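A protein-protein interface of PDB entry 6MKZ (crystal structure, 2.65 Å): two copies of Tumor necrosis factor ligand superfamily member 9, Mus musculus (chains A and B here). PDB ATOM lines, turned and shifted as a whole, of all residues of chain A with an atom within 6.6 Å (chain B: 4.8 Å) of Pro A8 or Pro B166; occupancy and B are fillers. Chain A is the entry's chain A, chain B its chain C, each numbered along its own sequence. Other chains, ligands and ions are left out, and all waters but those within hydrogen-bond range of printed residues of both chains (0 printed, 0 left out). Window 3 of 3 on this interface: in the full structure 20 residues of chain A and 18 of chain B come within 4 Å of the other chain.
The backbone carbonyl oxygen (O) of Val A9 sits at hydrogen-bond distance from the backbone NH (N) of Leu A163, 3.0 Å away.
The side-chain hydroxyl of Ser A40 sits at hydrogen-bond distance from the backbone NH of Phe A10 (2.8 Å).
Leu B163 touches Pro A8.
CB of Pro A8 touches O of Val B164, 3.3 Å away.
CD of Pro A8 touches CD of Pro B166, 3.8 Å away.
Val A9 touches Phe B162 (O to CE2, 3.9 Å).
Phe A10 touches Val B164 (CD2 to CG2, 3.6 Å).
Val B164 touches Tyr A38.
Leu A163 touches Phe B162.
Pro A8 touches three residues of chain B.
Pro B166 touches one residue of chain A.
Of the printed residues of chain A, Leu B163 touches Pro A8.
Of the printed residues of chain A, Val B164 touches Pro A8, Phe A10 and Tyr A38.
Of the printed residues of chain B, Tyr A38 touches Val B164 (3.8 Å).
Of the printed residues of chain B, Phe A10 touches Val B164 (3.6 Å).
Gln A41 touches none of the printed residues of chain B.
Ser A7 touches none of the printed residues of chain B.
Hydrophobic or aromatic side chains of chain A that line the printed part of chain B: Pro A8, Phe A10 and Tyr A38.
Hydrophobic or aromatic side chains of chain B that line the printed part of chain A: Phe B162, Val B164 and Pro B166.
Among the printed residues, no Asp or Glu carboxylate lies within 4 Å of a Lys or Arg side-chain nitrogen of the other chain.
Position printed for both chains: 163.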
ATOM      1  N   GLY A   6      10.493 -27.734 -10.411  1.00  0.00           N
ATOM      2  CA  GLY A   6       9.478 -28.176 -11.357  1.00  0.00           C
ATOM      3  C   GLY A   6       8.085 -28.198 -10.762  1.00  0.00           C
ATOM      4  O   GLY A   6       7.729 -27.302  -9.990  1.00  0.00           O
ATOM      5  N   SER A   7       7.290 -29.231 -11.110  1.00  0.00           N
ATOM      6  CA  SER A   7       5.907 -29.415 -10.663  1.00  0.00           C
ATOM      7  C   SER A   7       5.809 -29.740  -9.157  1.00  0.00           C
ATOM      8  O   SER A   7       6.689 -30.435  -8.646  1.00  0.00           O
ATOM      9  CB  SER A   7       5.240 -30.520 -11.475  1.00  0.00           C
ATOM     10  OG  SER A   7       5.174 -30.144 -12.840  1.00  0.00           O
ATOM     11  N   PRO A   8       4.748 -29.268  -8.442  1.00  0.00           N
ATOM     12  CA  PRO A   8       4.624 -29.567  -7.003  1.00  0.00           C
ATOM     13  C   PRO A   8       4.462 -31.048  -6.699  1.00  0.00           C
ATOM     14  O   PRO A   8       3.822 -31.763  -7.469  1.00  0.00           O
ATOM     15  CB  PRO A   8       3.360 -28.820  -6.596  1.00  0.00           C
ATOM     16  CG  PRO A   8       3.199 -27.758  -7.628  1.00  0.00           C
ATOM     17  CD  PRO A   8       3.641 -28.403  -8.889  1.00  0.00           C
ATOM     18  N   VAL A   9       5.051 -31.503  -5.580  1.00  0.00           N
ATOM     19  CA  VAL A   9       4.985 -32.898  -5.167  1.00  0.00           C
ATOM     20  C   VAL A   9       3.991 -32.970  -4.012  1.00  0.00           C
ATOM     21  O   VAL A   9       4.229 -32.384  -2.954  1.00  0.00           O
ATOM     22  CB  VAL A   9       6.383 -33.470  -4.824  1.00  0.00           C
ATOM     23  CG1 VAL A   9       6.281 -34.842  -4.200  1.00  0.00           C
ATOM     24  CG2 VAL A   9       7.270 -33.539  -6.049  1.00  0.00           C
ATOM     25  N   PHE A  10       2.859 -33.660  -4.234  1.00  0.00           N
ATOM     26  CA  PHE A  10       1.797 -33.791  -3.252  1.00  0.00           C
ATOM     27  C   PHE A  10       1.091 -35.133  -3.340  1.00  0.00           C
ATOM     28  O   PHE A  10       0.838 -35.621  -4.432  1.00  0.00           O
ATOM     29  CB  PHE A  10       0.764 -32.647  -3.443  1.00  0.00           C
ATOM     30  CG  PHE A  10      -0.524 -32.803  -2.647  1.00  0.00           C
ATOM     31  CD1 PHE A  10      -0.529 -32.672  -1.268  1.00  0.00           C
ATOM     32  CD2 PHE A  10      -1.721 -33.107  -3.280  1.00  0.00           C
ATOM     33  CE1 PHE A  10      -1.714 -32.840  -0.538  1.00  0.00           C
ATOM     34  CE2 PHE A  10      -2.905 -33.263  -2.552  1.00  0.00           C
ATOM     35  CZ  PHE A  10      -2.890 -33.137  -1.191  1.00  0.00           C
ATOM     36  N   TYR A  38      -5.158 -38.549  -4.258  1.00  0.00           N
ATOM     37  CA  TYR A  38      -4.305 -37.831  -5.190  1.00  0.00           C
ATOM     38  C   TYR A  38      -2.862 -38.280  -5.009  1.00  0.00           C
ATOM     39  O   TYR A  38      -2.390 -38.397  -3.879  1.00  0.00           O
ATOM     40  CB  TYR A  38      -4.432 -36.309  -4.977  1.00  0.00           C
ATOM     41  CG  TYR A  38      -3.683 -35.475  -5.997  1.00  0.00           C
ATOM     42  CD1 TYR A  38      -2.341 -35.149  -5.810  1.00  0.00           C
ATOM     43  CD2 TYR A  38      -4.313 -35.001  -7.139  1.00  0.00           C
ATOM     44  CE1 TYR A  38      -1.644 -34.387  -6.747  1.00  0.00           C
ATOM     45  CE2 TYR A  38      -3.622 -34.249  -8.089  1.00  0.00           C
ATOM     46  CZ  TYR A  38      -2.289 -33.943  -7.889  1.00  0.00           C
ATOM     47  OH  TYR A  38      -1.612 -33.206  -8.828  1.00  0.00           O
ATOM     48  N   SER A  40       0.741 -37.152  -7.026  1.00  0.00           N
ATOM     49  CA  SER A  40       1.423 -36.346  -8.039  1.00  0.00           C
ATOM     50  C   SER A  40       2.622 -37.125  -8.663  1.00  0.00           C
ATOM     51  O   SER A  40       2.870 -38.281  -8.313  1.00  0.00           O
ATOM     52  CB  SER A  40       1.893 -35.020  -7.440  1.00  0.00           C
ATOM     53  OG  SER A  40       3.038 -35.191  -6.621  1.00  0.00           O
ATOM     54  N   GLN A  41       3.338 -36.496  -9.614  1.00  0.00           N
ATOM     55  CA  GLN A  41       4.550 -37.043 -10.224  1.00  0.00           C
ATOM     56  C   GLN A  41       5.686 -36.937  -9.193  1.00  0.00           C
ATOM     57  O   GLN A  41       5.662 -36.024  -8.357  1.00  0.00           O
ATOM     58  CB  GLN A  41       4.893 -36.276 -11.512  1.00  0.00           C
ATOM     59  N   LEU A 163       6.107 -31.636  -0.707  1.00  0.00           N
ATOM     60  CA  LEU A 163       7.491 -31.169  -0.702  1.00  0.00           C
ATOM     61  C   LEU A 163       7.509 -29.656  -0.472  1.00  0.00           C
ATOM     62  O   LEU A 163       7.108 -28.903  -1.352  1.00  0.00           O
ATOM     63  CB  LEU A 163       8.185 -31.581  -2.014  1.00  0.00           C
ATOM     64  CG  LEU A 163       9.625 -31.124  -2.260  1.00  0.00           C
ATOM     65  CD1 LEU A 163      10.589 -31.680  -1.226  1.00  0.00           C
ATOM     66  CD2 LEU A 163      10.080 -31.516  -3.645  1.00  0.00           C
ATOM     67  N   PRO B  57      -2.198 -17.960  -9.277  1.00  0.00           N
ATOM     68  CA  PRO B  57      -3.413 -18.796  -9.313  1.00  0.00           C
ATOM     69  C   PRO B  57      -3.095 -20.283  -9.504  1.00  0.00           C
ATOM     70  O   PRO B  57      -2.064 -20.636 -10.066  1.00  0.00           O
ATOM     71  CB  PRO B  57      -4.190 -18.236 -10.509  1.00  0.00           C
ATOM     72  CG  PRO B  57      -3.146 -17.670 -11.407  1.00  0.00           C
ATOM     73  CD  PRO B  57      -1.945 -17.308 -10.583  1.00  0.00           C
ATOM     74  N   GLY B  58      -4.008 -21.136  -9.074  1.00  0.00           N
ATOM     75  CA  GLY B  58      -3.880 -22.580  -9.216  1.00  0.00           C
ATOM     76  C   GLY B  58      -4.722 -23.354  -8.231  1.00  0.00           C
ATOM     77  O   GLY B  58      -5.507 -22.766  -7.475  1.00  0.00           O
ATOM     78  N   PHE B 162      -0.991 -25.109   0.401  1.00  0.00           N
ATOM     79  CA  PHE B 162       0.063 -25.566  -0.480  1.00  0.00           C
ATOM     80  C   PHE B 162      -0.475 -25.498  -1.915  1.00  0.00           C
ATOM     81  O   PHE B 162      -1.663 -25.744  -2.106  1.00  0.00           O
ATOM     82  CB  PHE B 162       0.484 -26.999  -0.094  1.00  0.00           C
ATOM     83  CG  PHE B 162       1.662 -27.544  -0.868  1.00  0.00           C
ATOM     84  CD1 PHE B 162       2.961 -27.143  -0.569  1.00  0.00           C
ATOM     85  CD2 PHE B 162       1.476 -28.445  -1.908  1.00  0.00           C
ATOM     86  CE1 PHE B 162       4.050 -27.656  -1.284  1.00  0.00           C
ATOM     87  CE2 PHE B 162       2.566 -28.920  -2.654  1.00  0.00           C
ATOM     88  CZ  PHE B 162       3.841 -28.540  -2.324  1.00  0.00           C
ATOM     89  N   LEU B 163       0.352 -25.055  -2.890  1.00  0.00           N
ATOM     90  CA  LEU B 163      -0.019 -25.021  -4.297  1.00  0.00           C
ATOM     91  C   LEU B 163       0.278 -26.408  -4.881  1.00  0.00           C
ATOM     92  O   LEU B 163       1.438 -26.773  -5.001  1.00  0.00           O
ATOM     93  CB  LEU B 163       0.722 -23.888  -5.039  1.00  0.00           C
ATOM     94  CG  LEU B 163       0.551 -23.767  -6.556  1.00  0.00           C
ATOM     95  CD1 LEU B 163      -0.885 -23.485  -6.952  1.00  0.00           C
ATOM     96  CD2 LEU B 163       1.447 -22.682  -7.099  1.00  0.00           C
ATOM     97  N   VAL B 164      -0.780 -27.197  -5.166  1.00  0.00           N
ATOM     98  CA  VAL B 164      -0.713 -28.575  -5.676  1.00  0.00           C
ATOM     99  C   VAL B 164      -0.503 -28.590  -7.208  1.00  0.00           C
ATOM    100  O   VAL B 164       0.280 -29.400  -7.721  1.00  0.00           O
ATOM    101  CB  VAL B 164      -1.975 -29.363  -5.246  1.00  0.00           C
ATOM    102  CG1 VAL B 164      -2.065 -30.709  -5.947  1.00  0.00           C
ATOM    103  CG2 VAL B 164      -1.975 -29.561  -3.742  1.00  0.00           C
ATOM    104  N   LYS B 165      -1.221 -27.724  -7.929  1.00  0.00           N
ATOM    105  CA  LYS B 165      -1.089 -27.620  -9.373  1.00  0.00           C
ATOM    106  C   LYS B 165      -1.259 -26.167  -9.804  1.00  0.00           C
ATOM    107  O   LYS B 165      -2.370 -25.643  -9.700  1.00  0.00           O
ATOM    108  CB  LYS B 165      -2.102 -28.537 -10.101  1.00  0.00           C
ATOM    109  N   PRO B 166      -0.181 -25.484 -10.254  1.00  0.00           N
ATOM    110  CA  PRO B 166      -0.343 -24.101 -10.759  1.00  0.00           C
ATOM    111  C   PRO B 166      -1.108 -24.101 -12.079  1.00  0.00           C
ATOM    112  O   PRO B 166      -0.981 -25.060 -12.852  1.00  0.00           O
ATOM    113  CB  PRO B 166       1.099 -23.613 -10.963  1.00  0.00           C
ATOM    114  CG  PRO B 166       1.982 -24.681 -10.332  1.00  0.00           C
ATOM    115  CD  PRO B 166       1.204 -25.951 -10.430  1.00  0.00           C
ATOM    116  N   ASP B 167      -1.903 -23.048 -12.339  1.00  0.00           N
ATOM    117  CA  ASP B 167      -2.699 -22.985 -13.574  1.00  0.00           C
ATOM    118  C   ASP B 167      -1.857 -22.713 -14.814  1.00  0.00           C
ATOM    119  O   ASP B 167      -0.845 -22.008 -14.751  1.00  0.00           O
ATOM    120  CB  ASP B 167      -3.826 -21.938 -13.474  1.00  0.00           C
ATOM    121  CG  ASP B 167      -5.043 -22.396 -12.690  1.00  0.00           C
ATOM    122  OD1 ASP B 167      -5.065 -23.577 -12.250  1.00  0.00           O
ATOM    123  OD2 ASP B 167      -5.977 -21.581 -12.515  1.00  0.00           O
ATOM    124  N   ASN B 168      -2.358 -23.240 -15.972  1.00  0.00           N
ATOM    125  CA  ASN B 168      -1.824 -23.107 -17.342  1.00  0.00           C
ATOM    126  C   ASN B 168      -2.820 -23.718 -18.334  1.00  0.00           C
ATOM    127  O   ASN B 168      -2.579 -23.753 -19.541  1.00  0.00           O
ATOM    128  CB  ASN B 168      -0.440 -23.767 -17.487  1.00  0.00           C
ATOM    129  CG  ASN B 168       0.471 -23.134 -18.516  1.00  0.00           C
ATOM    130  OD1 ASN B 168       0.043 -22.435 -19.447  1.00  0.00           O
ATOM    131  ND2 ASN B 168       1.765 -23.381 -18.378  1.00  0.00           N
